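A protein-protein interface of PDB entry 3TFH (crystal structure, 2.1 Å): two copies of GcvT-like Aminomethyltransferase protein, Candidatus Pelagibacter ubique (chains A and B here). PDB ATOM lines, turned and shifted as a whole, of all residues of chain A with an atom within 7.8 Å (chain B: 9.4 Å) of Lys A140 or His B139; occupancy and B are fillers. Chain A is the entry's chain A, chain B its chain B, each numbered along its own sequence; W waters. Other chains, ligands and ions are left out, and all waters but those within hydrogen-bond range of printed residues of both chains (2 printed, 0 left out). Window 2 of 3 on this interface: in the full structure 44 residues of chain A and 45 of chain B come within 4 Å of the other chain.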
ATOM      1  N   ASP A  72      21.287 -23.762   7.519  1.00  0.00           N
ATOM      2  CA  ASP A  72      20.876 -23.544   6.132  1.00  0.00           C
ATOM      3  C   ASP A  72      20.617 -22.067   5.751  1.00  0.00           C
ATOM      4  O   ASP A  72      20.090 -21.763   4.653  1.00  0.00           O
ATOM      5  CB  ASP A  72      19.682 -24.460   5.851  1.00  0.00           C
ATOM      6  CG  ASP A  72      20.090 -25.964   5.838  1.00  0.00           C
ATOM      7  OD1 ASP A  72      21.216 -26.254   5.313  1.00  0.00           O
ATOM      8  OD2 ASP A  72      19.297 -26.805   6.337  1.00  0.00           O
ATOM      9  N   GLU A 101       8.891 -17.638  -8.104  1.00  0.00           N
ATOM     10  CA  GLU A 101       8.912 -18.751  -9.085  1.00  0.00           C
ATOM     11  C   GLU A 101       8.761 -18.288 -10.539  1.00  0.00           C
ATOM     12  O   GLU A 101       9.164 -19.019 -11.459  1.00  0.00           O
ATOM     13  CB  GLU A 101       7.896 -19.855  -8.747  1.00  0.00           C
ATOM     14  CG  GLU A 101       8.516 -21.050  -7.989  1.00  0.00           C
ATOM     15  CD  GLU A 101       7.644 -22.320  -8.024  1.00  0.00           C
ATOM     16  OE1 GLU A 101       7.941 -23.217  -8.824  1.00  0.00           O
ATOM     17  OE2 GLU A 101       6.669 -22.439  -7.257  1.00  0.00           O
ATOM     18  N   GLY A 134       8.086 -19.152   4.502  1.00  0.00           N
ATOM     19  CA  GLY A 134       7.412 -20.023   3.534  1.00  0.00           C
ATOM     20  C   GLY A 134       8.420 -20.960   2.867  1.00  0.00           C
ATOM     21  O   GLY A 134       8.240 -22.167   2.928  1.00  0.00           O
ATOM     22  N   LEU A 135       9.462 -20.389   2.263  1.00  0.00           N
ATOM     23  CA  LEU A 135      10.534 -21.141   1.627  1.00  0.00           C
ATOM     24  C   LEU A 135      11.285 -22.094   2.571  1.00  0.00           C
ATOM     25  O   LEU A 135      11.542 -23.236   2.191  1.00  0.00           O
ATOM     26  CB  LEU A 135      11.576 -20.239   0.993  1.00  0.00           C
ATOM     27  CG  LEU A 135      11.223 -19.520  -0.289  1.00  0.00           C
ATOM     28  CD1 LEU A 135      12.237 -18.467  -0.474  1.00  0.00           C
ATOM     29  CD2 LEU A 135      11.129 -20.462  -1.518  1.00  0.00           C
ATOM     30  N   ALA A 136      11.596 -21.636   3.786  1.00  0.00           N
ATOM     31  CA  ALA A 136      12.241 -22.464   4.812  1.00  0.00           C
ATOM     32  C   ALA A 136      11.447 -23.745   5.157  1.00  0.00           C
ATOM     33  O   ALA A 136      11.996 -24.875   5.158  1.00  0.00           O
ATOM     34  CB  ALA A 136      12.534 -21.641   6.080  1.00  0.00           C
ATOM     35  N   SER A 137      10.169 -23.590   5.457  1.00  0.00           N
ATOM     36  CA  SER A 137       9.317 -24.718   5.702  1.00  0.00           C
ATOM     37  C   SER A 137       9.176 -25.625   4.458  1.00  0.00           C
ATOM     38  O   SER A 137       9.290 -26.842   4.555  1.00  0.00           O
ATOM     39  CB  SER A 137       7.950 -24.240   6.136  1.00  0.00           C
ATOM     40  OG  SER A 137       7.049 -25.320   6.189  1.00  0.00           O
ATOM     41  N   GLY A 138       8.916 -25.037   3.292  1.00  0.00           N
ATOM     42  CA  GLY A 138       8.707 -25.830   2.071  1.00  0.00           C
ATOM     43  C   GLY A 138       9.923 -26.647   1.575  1.00  0.00           C
ATOM     44  O   GLY A 138       9.798 -27.785   1.106  1.00  0.00           O
ATOM     45  N   HIS A 139      11.082 -26.013   1.610  1.00  0.00           N
ATOM     46  CA  HIS A 139      12.376 -26.644   1.341  1.00  0.00           C
ATOM     47  C   HIS A 139      12.996 -27.348   2.556  1.00  0.00           C
ATOM     48  O   HIS A 139      14.095 -27.800   2.427  1.00  0.00           O
ATOM     49  CB  HIS A 139      13.368 -25.600   0.832  1.00  0.00           C
ATOM     50  CG  HIS A 139      13.107 -25.140  -0.568  1.00  0.00           C
ATOM     51  ND1 HIS A 139      12.092 -24.265  -0.897  1.00  0.00           N
ATOM     52  CD2 HIS A 139      13.711 -25.461  -1.726  1.00  0.00           C
ATOM     53  CE1 HIS A 139      12.102 -24.053  -2.195  1.00  0.00           C
ATOM     54  NE2 HIS A 139      13.059 -24.790  -2.726  1.00  0.00           N
ATOM     55  N   LYS A 140      12.276 -27.458   3.678  1.00  0.00           N
ATOM     56  CA  LYS A 140      12.754 -28.168   4.870  1.00  0.00           C
ATOM     57  C   LYS A 140      14.175 -27.719   5.334  1.00  0.00           C
ATOM     58  O   LYS A 140      15.071 -28.565   5.561  1.00  0.00           O
ATOM     59  CB  LYS A 140      12.628 -29.699   4.610  1.00  0.00           C
ATOM     60  CG  LYS A 140      11.238 -30.078   3.940  1.00  0.00           C
ATOM     61  CD  LYS A 140      10.899 -31.576   3.914  1.00  0.00           C
ATOM     62  CE  LYS A 140       9.412 -31.857   4.144  1.00  0.00           C
ATOM     63  NZ  LYS A 140       8.592 -31.703   2.927  1.00  0.00           N
ATOM     64  N   PHE A 141      14.391 -26.392   5.459  1.00  0.00           N
ATOM     65  CA  PHE A 141      15.687 -25.835   5.898  1.00  0.00           C
ATOM     66  C   PHE A 141      15.737 -25.722   7.400  1.00  0.00           C
ATOM     67  O   PHE A 141      14.742 -25.486   8.048  1.00  0.00           O
ATOM     68  CB  PHE A 141      16.025 -24.443   5.292  1.00  0.00           C
ATOM     69  CG  PHE A 141      16.320 -24.452   3.842  1.00  0.00           C
ATOM     70  CD1 PHE A 141      17.179 -25.371   3.293  1.00  0.00           C
ATOM     71  CD2 PHE A 141      15.740 -23.507   3.004  1.00  0.00           C
ATOM     72  CE1 PHE A 141      17.444 -25.384   1.947  1.00  0.00           C
ATOM     73  CE2 PHE A 141      16.005 -23.501   1.664  1.00  0.00           C
ATOM     74  CZ  PHE A 141      16.874 -24.451   1.121  1.00  0.00           C
ATOM     75  N   ASP A 142      16.937 -25.906   7.940  1.00  0.00           N
ATOM     76  CA  ASP A 142      17.215 -25.734   9.351  1.00  0.00           C
ATOM     77  C   ASP A 142      17.758 -24.307   9.524  1.00  0.00           C
ATOM     78  O   ASP A 142      18.950 -24.036   9.332  1.00  0.00           O
ATOM     79  CB  ASP A 142      18.290 -26.759   9.744  1.00  0.00           C
ATOM     80  CG  ASP A 142      18.549 -26.831  11.210  1.00  0.00           C
ATOM     81  OD1 ASP A 142      19.598 -27.404  11.541  1.00  0.00           O
ATOM     82  OD2 ASP A 142      17.744 -26.338  12.022  1.00  0.00           O
ATOM     83  N   VAL A 143      16.850 -23.397   9.880  1.00  0.00           N
ATOM     84  CA  VAL A 143      17.180 -21.982  10.094  1.00  0.00           C
ATOM     85  C   VAL A 143      16.343 -21.440  11.231  1.00  0.00           C
ATOM     86  O   VAL A 143      15.409 -22.102  11.691  1.00  0.00           O
ATOM     87  CB  VAL A 143      16.963 -21.141   8.820  1.00  0.00           C
ATOM     88  CG1 VAL A 143      17.878 -21.570   7.740  1.00  0.00           C
ATOM     89  CG2 VAL A 143      15.453 -21.188   8.347  1.00  0.00           C
ATOM     90  N   ASP B  72      -3.091 -28.677  -6.745  1.00  0.00           N
ATOM     91  CA  ASP B  72      -2.697 -28.677  -5.337  1.00  0.00           C
ATOM     92  C   ASP B  72      -3.167 -27.452  -4.521  1.00  0.00           C
ATOM     93  O   ASP B  72      -2.654 -27.209  -3.419  1.00  0.00           O
ATOM     94  CB  ASP B  72      -1.169 -28.856  -5.168  1.00  0.00           C
ATOM     95  CG  ASP B  72      -0.666 -30.203  -5.728  1.00  0.00           C
ATOM     96  OD1 ASP B  72      -1.370 -31.229  -5.523  1.00  0.00           O
ATOM     97  OD2 ASP B  72       0.429 -30.211  -6.356  1.00  0.00           O
ATOM     98  N   GLU B  75      -4.828 -28.246  -0.874  1.00  0.00           N
ATOM     99  CA  GLU B  75      -3.754 -28.717   0.053  1.00  0.00           C
ATOM    100  C   GLU B  75      -2.878 -27.567   0.533  1.00  0.00           C
ATOM    101  O   GLU B  75      -2.587 -27.491   1.739  1.00  0.00           O
ATOM    102  CB  GLU B  75      -2.860 -29.739  -0.638  1.00  0.00           C
ATOM    103  CG  GLU B  75      -1.721 -30.197   0.227  1.00  0.00           C
ATOM    104  CD  GLU B  75      -0.949 -31.364  -0.328  1.00  0.00           C
ATOM    105  OE1 GLU B  75      -1.184 -31.851  -1.485  1.00  0.00           O
ATOM    106  OE2 GLU B  75      -0.074 -31.766   0.435  1.00  0.00           O
ATOM    107  N   LEU B  76      -2.462 -26.680  -0.392  1.00  0.00           N
ATOM    108  CA  LEU B  76      -1.667 -25.482  -0.021  1.00  0.00           C
ATOM    109  C   LEU B  76      -2.419 -24.574   0.891  1.00  0.00           C
ATOM    110  O   LEU B  76      -1.885 -24.108   1.882  1.00  0.00           O
ATOM    111  CB  LEU B  76      -1.205 -24.689  -1.220  1.00  0.00           C
ATOM    112  CG  LEU B  76      -0.461 -23.356  -0.993  1.00  0.00           C
ATOM    113  CD1 LEU B  76       0.791 -23.568  -0.073  1.00  0.00           C
ATOM    114  CD2 LEU B  76      -0.051 -22.799  -2.349  1.00  0.00           C
ATOM    115  N   LEU B  79      -2.499 -26.264   4.356  1.00  0.00           N
ATOM    116  CA  LEU B  79      -1.149 -26.228   4.948  1.00  0.00           C
ATOM    117  C   LEU B  79      -0.835 -24.900   5.711  1.00  0.00           C
ATOM    118  O   LEU B  79      -0.048 -24.883   6.643  1.00  0.00           O
ATOM    119  CB  LEU B  79      -0.106 -26.428   3.850  1.00  0.00           C
ATOM    120  CG  LEU B  79       1.364 -26.495   4.257  1.00  0.00           C
ATOM    121  CD1 LEU B  79       1.578 -27.712   5.122  1.00  0.00           C
ATOM    122  CD2 LEU B  79       2.283 -26.477   3.045  1.00  0.00           C
ATOM    123  N   MET B  80      -1.467 -23.809   5.305  1.00  0.00           N
ATOM    124  CA  MET B  80      -1.198 -22.503   5.882  1.00  0.00           C
ATOM    125  C   MET B  80      -2.009 -22.280   7.140  1.00  0.00           C
ATOM    126  O   MET B  80      -1.638 -21.423   7.918  1.00  0.00           O
ATOM    127  CB  MET B  80      -1.486 -21.389   4.872  1.00  0.00           C
ATOM    128  CG  MET B  80      -0.487 -21.351   3.809  1.00  0.00           C
ATOM    129  SD  MET B  80      -0.556 -19.957   2.648  1.00  0.00           S
ATOM    130  CE  MET B  80      -2.097 -20.300   1.899  1.00  0.00           C
ATOM    131  N   PHE B 131       4.159 -15.932   1.582  1.00  0.00           N
ATOM    132  CA  PHE B 131       4.147 -17.125   2.432  1.00  0.00           C
ATOM    133  C   PHE B 131       3.662 -18.295   1.593  1.00  0.00           C
ATOM    134  O   PHE B 131       4.367 -19.319   1.548  1.00  0.00           O
ATOM    135  CB  PHE B 131       3.207 -16.911   3.618  1.00  0.00           C
ATOM    136  CG  PHE B 131       3.252 -17.961   4.702  1.00  0.00           C
ATOM    137  CD1 PHE B 131       4.425 -18.284   5.347  1.00  0.00           C
ATOM    138  CD2 PHE B 131       2.103 -18.552   5.133  1.00  0.00           C
ATOM    139  CE1 PHE B 131       4.430 -19.217   6.376  1.00  0.00           C
ATOM    140  CE2 PHE B 131       2.104 -19.481   6.139  1.00  0.00           C
ATOM    141  CZ  PHE B 131       3.264 -19.785   6.784  1.00  0.00           C
ATOM    142  N   ALA B 132       2.536 -18.099   0.867  1.00  0.00           N
ATOM    143  CA  ALA B 132       2.013 -19.112  -0.074  1.00  0.00           C
ATOM    144  C   ALA B 132       3.011 -19.516  -1.185  1.00  0.00           C
ATOM    145  O   ALA B 132       3.226 -20.712  -1.413  1.00  0.00           O
ATOM    146  CB  ALA B 132       0.681 -18.647  -0.673  1.00  0.00           C
ATOM    147  N   LYS B 133       3.611 -18.529  -1.857  1.00  0.00           N
ATOM    148  CA  LYS B 133       4.554 -18.741  -2.936  1.00  0.00           C
ATOM    149  C   LYS B 133       5.816 -19.459  -2.393  1.00  0.00           C
ATOM    150  O   LYS B 133       6.367 -20.332  -3.075  1.00  0.00           O
ATOM    151  CB  LYS B 133       4.972 -17.438  -3.618  1.00  0.00           C
ATOM    152  CG  LYS B 133       3.958 -16.766  -4.557  1.00  0.00           C
ATOM    153  CD  LYS B 133       4.463 -15.409  -5.010  1.00  0.00           C
ATOM    154  CE  LYS B 133       3.546 -14.753  -6.014  1.00  0.00           C
ATOM    155  NZ  LYS B 133       4.000 -15.036  -7.372  1.00  0.00           N
ATOM    156  N   GLY B 134       6.253 -19.087  -1.181  1.00  0.00           N
ATOM    157  CA  GLY B 134       7.365 -19.788  -0.495  1.00  0.00           C
ATOM    158  C   GLY B 134       7.026 -21.249  -0.217  1.00  0.00           C
ATOM    159  O   GLY B 134       7.788 -22.146  -0.579  1.00  0.00           O
ATOM    160  N   LEU B 135       5.901 -21.502   0.452  1.00  0.00           N
ATOM    161  CA  LEU B 135       5.434 -22.881   0.621  1.00  0.00           C
ATOM    162  C   LEU B 135       5.365 -23.668  -0.732  1.00  0.00           C
ATOM    163  O   LEU B 135       5.874 -24.799  -0.836  1.00  0.00           O
ATOM    164  CB  LEU B 135       4.137 -22.936   1.443  1.00  0.00           C
ATOM    165  CG  LEU B 135       4.273 -22.542   2.916  1.00  0.00           C
ATOM    166  CD1 LEU B 135       2.927 -22.153   3.514  1.00  0.00           C
ATOM    167  CD2 LEU B 135       5.003 -23.670   3.831  1.00  0.00           C
ATOM    168  N   ALA B 136       4.813 -23.059  -1.775  1.00  0.00           N
ATOM    169  CA  ALA B 136       4.517 -23.733  -3.040  1.00  0.00           C
ATOM    170  C   ALA B 136       5.796 -24.153  -3.772  1.00  0.00           C
ATOM    171  O   ALA B 136       5.821 -25.247  -4.393  1.00  0.00           O
ATOM    172  CB  ALA B 136       3.662 -22.860  -3.978  1.00  0.00           C
ATOM    173  N   SER B 137       6.816 -23.278  -3.714  1.00  0.00           N
ATOM    174  CA  SER B 137       8.142 -23.516  -4.289  1.00  0.00           C
ATOM    175  C   SER B 137       8.831 -24.771  -3.718  1.00  0.00           C
ATOM    176  O   SER B 137       9.380 -25.578  -4.445  1.00  0.00           O
ATOM    177  CB  SER B 137       9.038 -22.313  -3.947  1.00  0.00           C
ATOM    178  OG  SER B 137      10.306 -22.432  -4.516  1.00  0.00           O
ATOM    179  N   GLY B 138       8.826 -24.871  -2.397  1.00  0.00           N
ATOM    180  CA  GLY B 138       9.458 -25.980  -1.687  1.00  0.00           C
ATOM    181  C   GLY B 138       8.767 -27.304  -1.976  1.00  0.00           C
ATOM    182  O   GLY B 138       9.411 -28.260  -2.394  1.00  0.00           O
ATOM    183  N   HIS B 139       7.456 -27.328  -1.799  1.00  0.00           N
ATOM    184  CA  HIS B 139       6.662 -28.552  -2.012  1.00  0.00           C
ATOM    185  C   HIS B 139       6.434 -28.832  -3.527  1.00  0.00           C
ATOM    186  O   HIS B 139       5.838 -29.842  -3.864  1.00  0.00           O
ATOM    187  CB  HIS B 139       5.335 -28.461  -1.240  1.00  0.00           C
ATOM    188  CG  HIS B 139       5.467 -28.424   0.277  1.00  0.00           C
ATOM    189  ND1 HIS B 139       5.820 -29.522   1.033  1.00  0.00           N
ATOM    190  CD2 HIS B 139       5.238 -27.427   1.171  1.00  0.00           C
ATOM    191  CE1 HIS B 139       5.840 -29.202   2.316  1.00  0.00           C
ATOM    192  NE2 HIS B 139       5.492 -27.930   2.432  1.00  0.00           N
ATOM    193  N   LYS B 140       6.937 -27.955  -4.415  1.00  0.00           N
ATOM    194  CA  LYS B 140       6.694 -28.021  -5.862  1.00  0.00           C
ATOM    195  C   LYS B 140       5.212 -28.251  -6.178  1.00  0.00           C
ATOM    196  O   LYS B 140       4.864 -29.086  -7.034  1.00  0.00           O
ATOM    197  CB  LYS B 140       7.574 -29.114  -6.511  1.00  0.00           C
ATOM    198  CG  LYS B 140       9.071 -28.931  -6.233  1.00  0.00           C
ATOM    199  CD  LYS B 140       9.855 -30.189  -6.555  1.00  0.00           C
ATOM    200  CE  LYS B 140      11.343 -29.922  -6.505  1.00  0.00           C
ATOM    201  NZ  LYS B 140      12.007 -30.547  -7.660  1.00  0.00           N
ATOM    202  N   PHE B 141       4.337 -27.534  -5.471  1.00  0.00           N
ATOM    203  CA  PHE B 141       2.894 -27.681  -5.699  1.00  0.00           C
ATOM    204  C   PHE B 141       2.507 -27.244  -7.124  1.00  0.00           C
ATOM    205  O   PHE B 141       3.108 -26.314  -7.705  1.00  0.00           O
ATOM    206  CB  PHE B 141       2.095 -26.922  -4.675  1.00  0.00           C
ATOM    207  CG  PHE B 141       2.020 -27.565  -3.288  1.00  0.00           C
ATOM    208  CD1 PHE B 141       1.835 -28.941  -3.109  1.00  0.00           C
ATOM    209  CD2 PHE B 141       2.059 -26.751  -2.157  1.00  0.00           C
ATOM    210  CE1 PHE B 141       1.713 -29.481  -1.823  1.00  0.00           C
ATOM    211  CE2 PHE B 141       1.939 -27.257  -0.873  1.00  0.00           C
ATOM    212  CZ  PHE B 141       1.789 -28.672  -0.693  1.00  0.00           C
ATOM    213  N   ASP B 142       1.533 -27.954  -7.692  1.00  0.00           N
ATOM    214  CA  ASP B 142       0.958 -27.634  -8.970  1.00  0.00           C
ATOM    215  C   ASP B 142      -0.172 -26.609  -8.700  1.00  0.00           C
ATOM    216  O   ASP B 142      -1.314 -27.004  -8.438  1.00  0.00           O
ATOM    217  CB  ASP B 142       0.417 -28.940  -9.619  1.00  0.00           C
ATOM    218  CG  ASP B 142      -0.170 -28.715 -10.996  1.00  0.00           C
ATOM    219  OD1 ASP B 142      -0.676 -29.705 -11.584  1.00  0.00           O
ATOM    220  OD2 ASP B 142      -0.144 -27.568 -11.487  1.00  0.00           O
ATOM    221  N   VAL B 143       0.184 -25.311  -8.662  1.00  0.00           N
ATOM    222  CA  VAL B 143      -0.751 -24.237  -8.286  1.00  0.00           C
ATOM    223  C   VAL B 143      -0.399 -22.974  -9.029  1.00  0.00           C
ATOM    224  O   VAL B 143       0.695 -22.826  -9.536  1.00  0.00           O
ATOM    225  CB  VAL B 143      -0.818 -23.907  -6.736  1.00  0.00           C
ATOM    226  CG1 VAL B 143      -1.407 -25.015  -5.972  1.00  0.00           C
ATOM    227  CG2 VAL B 143       0.528 -23.481  -6.156  1.00  0.00           C
ATOM    228  N   ASN B 273      -3.037 -31.651   7.699  1.00  0.00           N
ATOM    229  CA  ASN B 273      -1.658 -31.230   7.767  1.00  0.00           C
ATOM    230  C   ASN B 273      -1.538 -29.674   7.640  1.00  0.00           C
ATOM    231  O   ASN B 273      -2.036 -29.063   6.657  1.00  0.00           O
ATOM    232  CB  ASN B 273      -0.861 -31.972   6.701  1.00  0.00           C
ATOM    233  CG  ASN B 273       0.626 -31.639   6.732  1.00  0.00           C
ATOM    234  OD1 ASN B 273       1.189 -31.265   7.784  1.00  0.00           O
ATOM    235  ND2 ASN B 273       1.272 -31.764   5.574  1.00  0.00           N
ATOM    236  N   PHE B 274      -0.927 -29.048   8.655  1.00  0.00           N
ATOM    237  CA  PHE B 274      -0.603 -27.593   8.599  1.00  0.00           C
ATOM    238  C   PHE B 274       0.688 -27.255   9.416  1.00  0.00           C
ATOM    239  O   PHE B 274       1.085 -28.022  10.306  1.00  0.00           O
ATOM    240  CB  PHE B 274      -1.837 -26.754   9.014  1.00  0.00           C
ATOM    241  CG  PHE B 274      -2.194 -26.844  10.466  1.00  0.00           C
ATOM    242  CD1 PHE B 274      -1.573 -26.031  11.394  1.00  0.00           C
ATOM    243  CD2 PHE B 274      -3.169 -27.721  10.909  1.00  0.00           C
ATOM    244  CE1 PHE B 274      -1.911 -26.103  12.735  1.00  0.00           C
ATOM    245  CE2 PHE B 274      -3.505 -27.823  12.265  1.00  0.00           C
ATOM    246  CZ  PHE B 274      -2.883 -27.021  13.178  1.00  0.00           C
ATOM    247  N   LEU B 275       1.358 -26.150   9.089  1.00  0.00           N
ATOM    248  CA  LEU B 275       2.580 -25.731   9.819  1.00  0.00           C
ATOM    249  C   LEU B 275       2.375 -25.499  11.302  1.00  0.00           C
ATOM    250  O   LEU B 275       1.328 -25.076  11.729  1.00  0.00           O
ATOM    251  CB  LEU B 275       3.158 -24.409   9.276  1.00  0.00           C
ATOM    252  CG  LEU B 275       4.066 -24.508   8.081  1.00  0.00           C
ATOM    253  CD1 LEU B 275       3.247 -24.917   6.890  1.00  0.00           C
ATOM    254  CD2 LEU B 275       4.758 -23.176   7.879  1.00  0.00           C
HETATM  255  O   HOH W   1       6.059 -20.345  -5.762  1.00  0.00           O
HETATM  256  O   HOH W   2       5.456 -27.136   4.766  1.00  0.00           O
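The backbone carbonyl oxygen (O) of Gly A134 is in hydrogen-bond range of the backbone NH (N) of Leu B135 (3.5 Å).
O of Leu A135 lies close to ND1 of His A139.
The backbone carbonyl oxygen (O) of Leu B79 sits at hydrogen-bond distance from the backbone NH (N) of Leu B275, 3.1 Å away.
The backbone carbonyl oxygen (O) of Ala B136 lies within hydrogen-bond range of the backbone NH (N) of Phe B141, 2.9 Å away.
Glu A101 touches Ala B136 (OE2 to C, 3.98 Å).
Glu A101 touches Ser B137.
Phe B131 touches Gly A134 (O to CA, 3.7 Å).
Gly A134 touches Gly B134.
Leu A135 touches Gly B134.
Leu A135 touches Ser B137 (CD2 to OG, 3.7 Å).
Leu B135 touches Ser A137 (CD2 to OG, 3.5 Å).
Gly B138 touches Gly A138 (C to O, 3.3 Å).
His B139 touches Gly A138.
His A139 touches Ser B137 (CE1 to OG, 3.4 Å).
Of the printed residues of chain B, Lys A140 touches His B139.
Of the printed residues of chain A, His B139 touches Gly A138 (3.8 Å) and Lys A140 (3.8 Å).
Of the printed residues of chain B, Gly A138 touches Gly B138 and His B139.
Gly B138 touches two residues of chain A.
Of the printed residues of chain A, Ala B136 touches Glu A101.
Of the printed residues of chain A, Leu B135 touches Gly A134 and Ser A137.
Of the printed residues of chain A, Leu B275 touches Ser A137.
Printed residues of chain B within 4 Å of Glu A101: Ala B136 and Ser B137.
Of the printed residues of chain B, Ser A137 touches Leu B135 and Leu B275.
Phe B141 touches none of the printed residues of chain A.
Met B80 touches none of the printed residues of chain A.
The nearest printed residue of chain B that does not touch Lys A140 is Gly B138 (6.2 Å).
The nearest printed residue of chain A that does not touch His B139 is Ser A137 (4.5 Å).
Of the 21 printed residues of chain B, 8 touch a printed residue of chain A.
Printed residues of chain B that touch a printed residue of chain A: Phe B131, Gly B134, Leu B135, Ala B136, Ser B137, Gly B138, His B139 and Leu B275.
Hydrophobic or aromatic side chains of chain B within 4 Å of the printed part of chain A: Phe B131, Leu B135, His B139 and Leu B275.
Gly A134 touches Leu B135, and with the chains exchanged Leu A135 touches Gly B134.
Gly A138 touches its own counterpart, Gly B138.
Gly A138 touches His B139, and with the chains exchanged His A139 touches Gly B138.
Lys A140 touches His B139, but with the chains exchanged His A139 does not touch Lys B140 (6.6 Å).
11 positions are printed for both chains.
Of the 14 pairs that touch across the chains among the printed residues, 8 have their exchanged pair printed and touching as well.
Water W2 bridges a ring nitrogen (NE2) of His B139 (2.5 Å) and the side-chain hydroxyl of Ser A137 (2.8 Å).
Water W1 bridges the side-chain carboxylate (OE2) of Glu A101 (2.6 Å) and the backbone carbonyl oxygen (O) of Lys B133 (2.7 Å).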
